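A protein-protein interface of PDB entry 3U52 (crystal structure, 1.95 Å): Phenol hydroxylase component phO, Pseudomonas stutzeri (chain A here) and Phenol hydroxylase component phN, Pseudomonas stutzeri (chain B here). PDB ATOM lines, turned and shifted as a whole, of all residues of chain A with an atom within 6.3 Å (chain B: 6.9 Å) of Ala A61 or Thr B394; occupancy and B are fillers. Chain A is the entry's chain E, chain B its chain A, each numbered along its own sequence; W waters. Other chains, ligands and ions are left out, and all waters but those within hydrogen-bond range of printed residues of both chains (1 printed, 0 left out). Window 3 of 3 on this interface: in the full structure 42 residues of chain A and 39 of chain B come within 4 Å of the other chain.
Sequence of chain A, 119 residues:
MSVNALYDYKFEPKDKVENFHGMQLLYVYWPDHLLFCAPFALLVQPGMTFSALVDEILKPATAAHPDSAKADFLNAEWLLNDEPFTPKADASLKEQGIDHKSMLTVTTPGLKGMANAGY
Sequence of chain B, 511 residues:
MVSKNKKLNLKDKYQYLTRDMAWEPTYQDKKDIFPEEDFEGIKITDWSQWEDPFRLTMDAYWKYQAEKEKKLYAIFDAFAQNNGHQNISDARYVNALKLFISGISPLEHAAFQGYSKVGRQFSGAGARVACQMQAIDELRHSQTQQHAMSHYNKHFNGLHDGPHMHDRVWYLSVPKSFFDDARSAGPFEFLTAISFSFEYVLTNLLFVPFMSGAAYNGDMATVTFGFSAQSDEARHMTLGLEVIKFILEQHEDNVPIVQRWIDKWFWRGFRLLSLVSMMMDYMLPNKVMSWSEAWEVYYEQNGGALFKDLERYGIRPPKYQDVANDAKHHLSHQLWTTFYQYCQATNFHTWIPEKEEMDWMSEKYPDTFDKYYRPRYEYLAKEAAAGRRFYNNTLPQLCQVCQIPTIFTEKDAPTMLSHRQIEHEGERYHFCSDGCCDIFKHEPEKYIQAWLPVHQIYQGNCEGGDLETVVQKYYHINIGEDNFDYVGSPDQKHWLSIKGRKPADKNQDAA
The backbone NH of Ala A41 lies within hydrogen-bond range of the backbone carbonyl oxygen of Leu B395, 2.8 Å away. O of Ala A41 is in hydrogen-bond range of OH of Tyr B458.
O of Gln B341 is in hydrogen-bond range of NE2 of Gln B344. The side-chain amide oxygen (OD1) of Asn B392 sits at hydrogen-bond distance from the backbone NH (N) of Thr B394 (3.0 Å). OH of Tyr B342 lies within hydrogen-bond range of O of Thr B394 (2.9 Å). The side-chain amide oxygen (OE1) of Gln B344 lies close to the backbone carbonyl oxygen (O) of Asn B392. O of Gln B341 is in hydrogen-bond range of N of Asn B392, at 2.8 Å. OH of Tyr B342 sits at hydrogen-bond distance from ND2 of Asn B392 (3.4 Å).
Of the printed residues of chain B, Phe A36 touches Gln B341 (3.6 Å) and Asn B392 (3.7 Å). Printed residues of chain B within 4 Å of Phe A40: Thr B394 (3.5 Å) and Leu B395 (3.6 Å). Of the printed residues of chain B, Ala A41 touches Leu B395, Pro B396 and Tyr B458. Of the printed residues of chain B, Ala A61 touches Thr B394. Of the printed residues of chain B, Ala A64 touches Phe B390. Of the printed residues of chain A, Gln B341 touches Phe A36 (3.6 Å). Asn B393 touches none of the printed residues of chain A. Of chain A, only Phe A40 (3.5 Å), Leu A42 (3.8 Å) and Ala A61 (3.6 Å) come within 4 Å of Thr B394. Leu B467 touches none of the printed residues of chain A. The nearest residue of chain B that does not touch Ala A61 is Asn B392 (5.2 Å). The nearest residue of chain A that does not touch Thr B394 is Ala A41 (4.3 Å). The nearest printed residue of chain B that does not touch Ala A41 is Thr B394 (4.3 Å).
Water W1 lies within hydrogen-bond range of the backbone carbonyl oxygen of Ala A61, the side-chain hydroxyl of Thr B394 and the side-chain amide oxygen of Asn B392.
Hydrophobic or aromatic side chains of chain B within 4 Å of the printed part of chain A: Phe B390 and Tyr B458. Of the 14 printed residues of chain A, 6 touch a printed residue of chain B. Printed residues of chain A that touch a printed residue of chain B: Phe A36, Phe A40, Ala A41, Leu A42, Ala A61 and Ala A64. Among the printed residues, 11 pairs touch across the chains. Among the printed residues, no Asp or Glu carboxylate lies within 4 Å of a Lys or Arg side-chain nitrogen of the other chain.
Among the printed residues, pairs that only touch across the chains: Phe A40 with Thr B394 (3.5 Å), Phe A36 with Gln B341 (3.6 Å), Ala A41 with Pro B396 (3.6 Å), Phe A40 with Leu B395 (3.6 Å), Ala A64 with Phe B390 (3.6 Å), Ala A61 with Thr B394 (3.6 Å), Phe A36 with Asn B392 (3.7 Å), Leu A42 with Tyr B458 (3.7 Å) and Leu A42 with Thr B394 (3.8 Å).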
ATOM      1  N   PHE A  36     -33.500   8.261  22.886  1.00  0.00           N
ATOM      2  CA  PHE A  36     -33.119   9.070  21.735  1.00  0.00           C
ATOM      3  C   PHE A  36     -33.835   8.340  20.612  1.00  0.00           C
ATOM      4  O   PHE A  36     -33.521   7.178  20.308  1.00  0.00           O
ATOM      5  CB  PHE A  36     -31.598   9.013  21.535  1.00  0.00           C
ATOM      6  CG  PHE A  36     -30.860   9.381  22.745  1.00  0.00           C
ATOM      7  CD1 PHE A  36     -30.172   8.412  23.473  1.00  0.00           C
ATOM      8  CD2 PHE A  36     -30.892  10.712  23.214  1.00  0.00           C
ATOM      9  CE1 PHE A  36     -29.517   8.755  24.652  1.00  0.00           C
ATOM     10  CE2 PHE A  36     -30.244  11.053  24.404  1.00  0.00           C
ATOM     11  CZ  PHE A  36     -29.545  10.063  25.116  1.00  0.00           C
ATOM     12  N   PHE A  40     -28.032   9.329  16.038  1.00  0.00           N
ATOM     13  CA  PHE A  40     -27.498  10.691  15.994  1.00  0.00           C
ATOM     14  C   PHE A  40     -26.875  10.956  14.660  1.00  0.00           C
ATOM     15  O   PHE A  40     -26.213  10.084  14.111  1.00  0.00           O
ATOM     16  CB  PHE A  40     -26.438  10.857  17.052  1.00  0.00           C
ATOM     17  CG  PHE A  40     -26.926  10.653  18.459  1.00  0.00           C
ATOM     18  CD1 PHE A  40     -27.994  11.390  18.972  1.00  0.00           C
ATOM     19  CD2 PHE A  40     -26.265   9.765  19.294  1.00  0.00           C
ATOM     20  CE1 PHE A  40     -28.410  11.231  20.287  1.00  0.00           C
ATOM     21  CE2 PHE A  40     -26.678   9.594  20.630  1.00  0.00           C
ATOM     22  CZ  PHE A  40     -27.758  10.327  21.110  1.00  0.00           C
ATOM     23  N   ALA A  41     -27.062  12.160  14.145  1.00  0.00           N
ATOM     24  CA  ALA A  41     -26.354  12.624  12.945  1.00  0.00           C
ATOM     25  C   ALA A  41     -25.350  13.649  13.408  1.00  0.00           C
ATOM     26  O   ALA A  41     -25.715  14.697  13.957  1.00  0.00           O
ATOM     27  CB  ALA A  41     -27.304  13.240  11.936  1.00  0.00           C
ATOM     28  N   LEU A  42     -24.077  13.328  13.229  1.00  0.00           N
ATOM     29  CA  LEU A  42     -23.000  14.191  13.708  1.00  0.00           C
ATOM     30  C   LEU A  42     -22.146  14.763  12.539  1.00  0.00           C
ATOM     31  O   LEU A  42     -22.037  14.133  11.465  1.00  0.00           O
ATOM     32  CB  LEU A  42     -22.122  13.393  14.678  1.00  0.00           C
ATOM     33  CG  LEU A  42     -22.883  12.564  15.723  1.00  0.00           C
ATOM     34  CD1 LEU A  42     -21.944  11.466  16.240  1.00  0.00           C
ATOM     35  CD2 LEU A  42     -23.343  13.441  16.868  1.00  0.00           C
ATOM     36  N   GLU A  56     -15.537  13.570  23.479  1.00  0.00           N
ATOM     37  CA  GLU A  56     -15.984  14.936  23.218  1.00  0.00           C
ATOM     38  C   GLU A  56     -17.406  15.025  22.623  1.00  0.00           C
ATOM     39  O   GLU A  56     -18.090  16.040  22.796  1.00  0.00           O
ATOM     40  CB  GLU A  56     -15.006  15.689  22.284  1.00  0.00           C
ATOM     41  CG  GLU A  56     -13.523  15.814  22.745  1.00  0.00           C
ATOM     42  CD  GLU A  56     -12.651  16.482  21.666  1.00  0.00           C
ATOM     43  OE1 GLU A  56     -11.401  16.503  21.805  1.00  0.00           O
ATOM     44  OE2 GLU A  56     -13.218  16.990  20.666  1.00  0.00           O
ATOM     45  N   ILE A  57     -17.817  13.993  21.893  1.00  0.00           N
ATOM     46  CA  ILE A  57     -19.104  14.013  21.185  1.00  0.00           C
ATOM     47  C   ILE A  57     -20.093  12.971  21.667  1.00  0.00           C
ATOM     48  O   ILE A  57     -21.200  13.333  22.085  1.00  0.00           O
ATOM     49  CB  ILE A  57     -18.942  13.940  19.660  1.00  0.00           C
ATOM     50  CG1 ILE A  57     -17.994  15.044  19.185  1.00  0.00           C
ATOM     51  CG2 ILE A  57     -20.298  14.123  18.963  1.00  0.00           C
ATOM     52  CD1 ILE A  57     -17.561  14.898  17.797  1.00  0.00           C
ATOM     53  N   LEU A  58     -19.709  11.699  21.651  1.00  0.00           N
ATOM     54  CA  LEU A  58     -20.654  10.633  22.010  1.00  0.00           C
ATOM     55  C   LEU A  58     -21.124  10.661  23.481  1.00  0.00           C
ATOM     56  O   LEU A  58     -22.313  10.563  23.785  1.00  0.00           O
ATOM     57  CB  LEU A  58     -20.084   9.275  21.598  1.00  0.00           C
ATOM     58  CG  LEU A  58     -21.075   8.127  21.473  1.00  0.00           C
ATOM     59  CD1 LEU A  58     -22.200   8.515  20.457  1.00  0.00           C
ATOM     60  CD2 LEU A  58     -20.357   6.817  21.063  1.00  0.00           C
ATOM     61  N   LYS A  59     -20.198  10.831  24.404  1.00  0.00           N
ATOM     62  CA  LYS A  59     -20.542  10.943  25.823  1.00  0.00           C
ATOM     63  C   LYS A  59     -21.518  12.121  26.171  1.00  0.00           C
ATOM     64  O   LYS A  59     -22.521  11.912  26.838  1.00  0.00           O
ATOM     65  CB  LYS A  59     -19.239  11.022  26.633  1.00  0.00           C
ATOM     66  CG  LYS A  59     -19.179  10.094  27.814  1.00  0.00           C
ATOM     67  CD  LYS A  59     -19.187   8.629  27.390  1.00  0.00           C
ATOM     68  CE  LYS A  59     -19.925   7.742  28.421  1.00  0.00           C
ATOM     69  NZ  LYS A  59     -19.751   8.065  29.885  1.00  0.00           N
ATOM     70  N   PRO A  60     -21.200  13.370  25.760  1.00  0.00           N
ATOM     71  CA  PRO A  60     -22.179  14.475  25.873  1.00  0.00           C
ATOM     72  C   PRO A  60     -23.541  14.248  25.214  1.00  0.00           C
ATOM     73  O   PRO A  60     -24.546  14.561  25.806  1.00  0.00           O
ATOM     74  CB  PRO A  60     -21.464  15.626  25.169  1.00  0.00           C
ATOM     75  CG  PRO A  60     -20.036  15.355  25.458  1.00  0.00           C
ATOM     76  CD  PRO A  60     -19.918  13.867  25.250  1.00  0.00           C
ATOM     77  N   ALA A  61     -23.554  13.715  23.996  1.00  0.00           N
ATOM     78  CA  ALA A  61     -24.803  13.417  23.260  1.00  0.00           C
ATOM     79  C   ALA A  61     -25.724  12.447  24.040  1.00  0.00           C
ATOM     80  O   ALA A  61     -26.973  12.540  23.971  1.00  0.00           O
ATOM     81  CB  ALA A  61     -24.456  12.842  21.861  1.00  0.00           C
ATOM     82  N   THR A  62     -25.134  11.532  24.809  1.00  0.00           N
ATOM     83  CA  THR A  62     -25.930  10.476  25.441  1.00  0.00           C
ATOM     84  C   THR A  62     -26.206  10.729  26.917  1.00  0.00           C
ATOM     85  O   THR A  62     -26.842   9.908  27.577  1.00  0.00           O
ATOM     86  CB  THR A  62     -25.286   9.063  25.301  1.00  0.00           C
ATOM     87  OG1 THR A  62     -24.026   9.045  25.973  1.00  0.00           O
ATOM     88  CG2 THR A  62     -25.075   8.660  23.855  1.00  0.00           C
ATOM     89  N   ALA A  63     -25.749  11.879  27.427  1.00  0.00           N
ATOM     90  CA  ALA A  63     -25.735  12.144  28.858  1.00  0.00           C
ATOM     91  C   ALA A  63     -27.097  12.080  29.531  1.00  0.00           C
ATOM     92  O   ALA A  63     -27.172  11.784  30.705  1.00  0.00           O
ATOM     93  CB  ALA A  63     -25.008  13.492  29.176  1.00  0.00           C
ATOM     94  N   ALA A  64     -28.177  12.314  28.779  1.00  0.00           N
ATOM     95  CA  ALA A  64     -29.535  12.337  29.353  1.00  0.00           C
ATOM     96  C   ALA A  64     -30.037  10.966  29.784  1.00  0.00           C
ATOM     97  O   ALA A  64     -30.979  10.876  30.566  1.00  0.00           O
ATOM     98  CB  ALA A  64     -30.535  12.964  28.374  1.00  0.00           C
ATOM     99  N   SER A  68     -25.744   6.235  30.508  1.00  0.00           N
ATOM    100  CA  SER A  68     -24.599   6.926  29.900  1.00  0.00           C
ATOM    101  C   SER A  68     -23.372   6.936  30.828  1.00  0.00           C
ATOM    102  O   SER A  68     -22.247   6.642  30.399  1.00  0.00           O
ATOM    103  CB  SER A  68     -24.962   8.371  29.578  1.00  0.00           C
ATOM    104  OG  SER A  68     -23.960   8.981  28.776  1.00  0.00           O
ATOM    105  N   GLN B 341     -39.273  15.111  22.274  1.00  0.00           N
ATOM    106  CA  GLN B 341     -37.856  15.430  22.551  1.00  0.00           C
ATOM    107  C   GLN B 341     -37.284  16.465  21.619  1.00  0.00           C
ATOM    108  O   GLN B 341     -36.251  17.071  21.904  1.00  0.00           O
ATOM    109  CB  GLN B 341     -37.016  14.150  22.512  1.00  0.00           C
ATOM    110  CG  GLN B 341     -36.827  13.558  21.112  1.00  0.00           C
ATOM    111  CD  GLN B 341     -36.321  12.146  21.172  1.00  0.00           C
ATOM    112  OE1 GLN B 341     -37.061  11.219  21.511  1.00  0.00           O
ATOM    113  NE2 GLN B 341     -35.049  11.971  20.900  1.00  0.00           N
ATOM    114  N   TYR B 342     -37.936  16.691  20.501  1.00  0.00           N
ATOM    115  CA  TYR B 342     -37.471  17.661  19.528  1.00  0.00           C
ATOM    116  C   TYR B 342     -38.365  18.923  19.422  1.00  0.00           C
ATOM    117  O   TYR B 342     -38.151  19.792  18.549  1.00  0.00           O
ATOM    118  CB  TYR B 342     -37.331  16.969  18.185  1.00  0.00           C
ATOM    119  CG  TYR B 342     -36.089  16.082  18.049  1.00  0.00           C
ATOM    120  CD1 TYR B 342     -36.177  14.858  17.408  1.00  0.00           C
ATOM    121  CD2 TYR B 342     -34.835  16.519  18.485  1.00  0.00           C
ATOM    122  CE1 TYR B 342     -35.077  14.049  17.235  1.00  0.00           C
ATOM    123  CE2 TYR B 342     -33.682  15.691  18.331  1.00  0.00           C
ATOM    124  CZ  TYR B 342     -33.829  14.479  17.684  1.00  0.00           C
ATOM    125  OH  TYR B 342     -32.780  13.659  17.425  1.00  0.00           O
ATOM    126  N   GLN B 344     -38.411  21.644  20.986  1.00  0.00           N
ATOM    127  CA  GLN B 344     -37.681  22.934  21.040  1.00  0.00           C
ATOM    128  C   GLN B 344     -37.529  23.511  19.605  1.00  0.00           C
ATOM    129  O   GLN B 344     -37.230  24.703  19.414  1.00  0.00           O
ATOM    130  CB  GLN B 344     -36.316  22.830  21.793  1.00  0.00           C
ATOM    131  CG  GLN B 344     -35.109  22.235  21.018  1.00  0.00           C
ATOM    132  CD  GLN B 344     -35.051  20.726  21.120  1.00  0.00           C
ATOM    133  OE1 GLN B 344     -33.976  20.123  21.114  1.00  0.00           O
ATOM    134  NE2 GLN B 344     -36.187  20.116  21.259  1.00  0.00           N
ATOM    135  N   PHE B 390     -36.988  16.501  29.485  1.00  0.00           N
ATOM    136  CA  PHE B 390     -36.071  16.026  28.439  1.00  0.00           C
ATOM    137  C   PHE B 390     -36.287  16.726  27.072  1.00  0.00           C
ATOM    138  O   PHE B 390     -37.395  16.677  26.509  1.00  0.00           O
ATOM    139  CB  PHE B 390     -36.200  14.480  28.296  1.00  0.00           C
ATOM    140  CG  PHE B 390     -35.382  13.879  27.138  1.00  0.00           C
ATOM    141  CD1 PHE B 390     -33.986  13.976  27.107  1.00  0.00           C
ATOM    142  CD2 PHE B 390     -36.019  13.151  26.117  1.00  0.00           C
ATOM    143  CE1 PHE B 390     -33.273  13.431  26.043  1.00  0.00           C
ATOM    144  CE2 PHE B 390     -35.274  12.558  25.062  1.00  0.00           C
ATOM    145  CZ  PHE B 390     -33.923  12.721  25.029  1.00  0.00           C
ATOM    146  N   TYR B 391     -35.228  17.384  26.584  1.00  0.00           N
ATOM    147  CA  TYR B 391     -35.081  17.761  25.189  1.00  0.00           C
ATOM    148  C   TYR B 391     -33.812  17.173  24.606  1.00  0.00           C
ATOM    149  O   TYR B 391     -32.754  17.160  25.262  1.00  0.00           O
ATOM    150  CB  TYR B 391     -35.030  19.262  24.998  1.00  0.00           C
ATOM    151  CG  TYR B 391     -36.291  19.988  25.410  1.00  0.00           C
ATOM    152  CD1 TYR B 391     -36.424  20.483  26.708  1.00  0.00           C
ATOM    153  CD2 TYR B 391     -37.348  20.196  24.499  1.00  0.00           C
ATOM    154  CE1 TYR B 391     -37.566  21.192  27.114  1.00  0.00           C
ATOM    155  CE2 TYR B 391     -38.499  20.889  24.902  1.00  0.00           C
ATOM    156  CZ  TYR B 391     -38.585  21.390  26.190  1.00  0.00           C
ATOM    157  OH  TYR B 391     -39.712  22.047  26.608  1.00  0.00           O
ATOM    158  N   ASN B 392     -33.925  16.635  23.395  1.00  0.00           N
ATOM    159  CA  ASN B 392     -32.770  16.020  22.746  1.00  0.00           C
ATOM    160  C   ASN B 392     -32.086  17.059  21.865  1.00  0.00           C
ATOM    161  O   ASN B 392     -32.630  17.474  20.852  1.00  0.00           O
ATOM    162  CB  ASN B 392     -33.207  14.791  21.939  1.00  0.00           C
ATOM    163  CG  ASN B 392     -32.048  14.053  21.296  1.00  0.00           C
ATOM    164  OD1 ASN B 392     -30.906  14.541  21.298  1.00  0.00           O
ATOM    165  ND2 ASN B 392     -32.341  12.915  20.674  1.00  0.00           N
ATOM    166  N   ASN B 393     -30.885  17.471  22.274  1.00  0.00           N
ATOM    167  CA  ASN B 393     -30.118  18.504  21.566  1.00  0.00           C
ATOM    168  C   ASN B 393     -29.183  18.017  20.458  1.00  0.00           C
ATOM    169  O   ASN B 393     -28.430  18.805  19.876  1.00  0.00           O
ATOM    170  CB  ASN B 393     -29.433  19.458  22.554  1.00  0.00           C
ATOM    171  CG  ASN B 393     -30.423  20.395  23.245  1.00  0.00           C
ATOM    172  OD1 ASN B 393     -30.502  20.421  24.462  1.00  0.00           O
ATOM    173  ND2 ASN B 393     -31.171  21.176  22.465  1.00  0.00           N
ATOM    174  N   THR B 394     -29.296  16.756  20.085  1.00  0.00           N
ATOM    175  CA  THR B 394     -28.521  16.258  18.957  1.00  0.00           C
ATOM    176  C   THR B 394     -29.436  15.945  17.795  1.00  0.00           C
ATOM    177  O   THR B 394     -30.456  15.305  17.978  1.00  0.00           O
ATOM    178  CB  THR B 394     -27.701  14.949  19.307  1.00  0.00           C
ATOM    179  OG1 THR B 394     -26.933  15.132  20.517  1.00  0.00           O
ATOM    180  CG2 THR B 394     -26.792  14.576  18.146  1.00  0.00           C
ATOM    181  N   LEU B 395     -29.049  16.381  16.595  1.00  0.00           N
ATOM    182  CA  LEU B 395     -29.834  16.163  15.385  1.00  0.00           C
ATOM    183  C   LEU B 395     -29.916  14.649  15.001  1.00  0.00           C
ATOM    184  O   LEU B 395     -28.936  13.896  15.165  1.00  0.00           O
ATOM    185  CB  LEU B 395     -29.248  16.966  14.204  1.00  0.00           C
ATOM    186  CG  LEU B 395     -29.306  18.504  14.247  1.00  0.00           C
ATOM    187  CD1 LEU B 395     -28.544  19.099  13.071  1.00  0.00           C
ATOM    188  CD2 LEU B 395     -30.725  18.967  14.188  1.00  0.00           C
ATOM    189  N   PRO B 396     -31.072  14.215  14.474  1.00  0.00           N
ATOM    190  CA  PRO B 396     -31.248  12.802  14.071  1.00  0.00           C
ATOM    191  C   PRO B 396     -30.901  12.470  12.620  1.00  0.00           C
ATOM    192  O   PRO B 396     -30.885  13.342  11.754  1.00  0.00           O
ATOM    193  CB  PRO B 396     -32.731  12.605  14.282  1.00  0.00           C
ATOM    194  CG  PRO B 396     -33.318  13.900  13.842  1.00  0.00           C
ATOM    195  CD  PRO B 396     -32.343  14.960  14.335  1.00  0.00           C
ATOM    196  N   TYR B 458     -26.204  21.280   8.625  1.00  0.00           N
ATOM    197  CA  TYR B 458     -24.768  21.007   8.718  1.00  0.00           C
ATOM    198  C   TYR B 458     -23.947  21.570   7.536  1.00  0.00           C
ATOM    199  O   TYR B 458     -22.791  21.921   7.731  1.00  0.00           O
ATOM    200  CB  TYR B 458     -24.491  19.506   8.867  1.00  0.00           C
ATOM    201  CG  TYR B 458     -24.679  18.929  10.263  1.00  0.00           C
ATOM    202  CD1 TYR B 458     -24.335  19.628  11.379  1.00  0.00           C
ATOM    203  CD2 TYR B 458     -25.193  17.639  10.427  1.00  0.00           C
ATOM    204  CE1 TYR B 458     -24.477  19.069  12.652  1.00  0.00           C
ATOM    205  CE2 TYR B 458     -25.343  17.071  11.664  1.00  0.00           C
ATOM    206  CZ  TYR B 458     -24.982  17.779  12.782  1.00  0.00           C
ATOM    207  OH  TYR B 458     -25.147  17.194  14.022  1.00  0.00           O
ATOM    208  N   LEU B 467     -28.398  26.091  16.938  1.00  0.00           N
ATOM    209  CA  LEU B 467     -29.754  25.715  16.619  1.00  0.00           C
ATOM    210  C   LEU B 467     -30.781  26.790  17.029  1.00  0.00           C
ATOM    211  O   LEU B 467     -31.788  26.964  16.381  1.00  0.00           O
ATOM    212  CB  LEU B 467     -30.022  24.203  16.901  1.00  0.00           C
ATOM    213  CG  LEU B 467     -28.927  23.247  16.230  1.00  0.00           C
ATOM    214  CD1 LEU B 467     -29.019  21.749  16.612  1.00  0.00           C
ATOM    215  CD2 LEU B 467     -28.727  23.314  14.730  1.00  0.00           C
HETATM  216  O   HOH W   1     -28.320  14.256  22.708  1.00  0.00           O
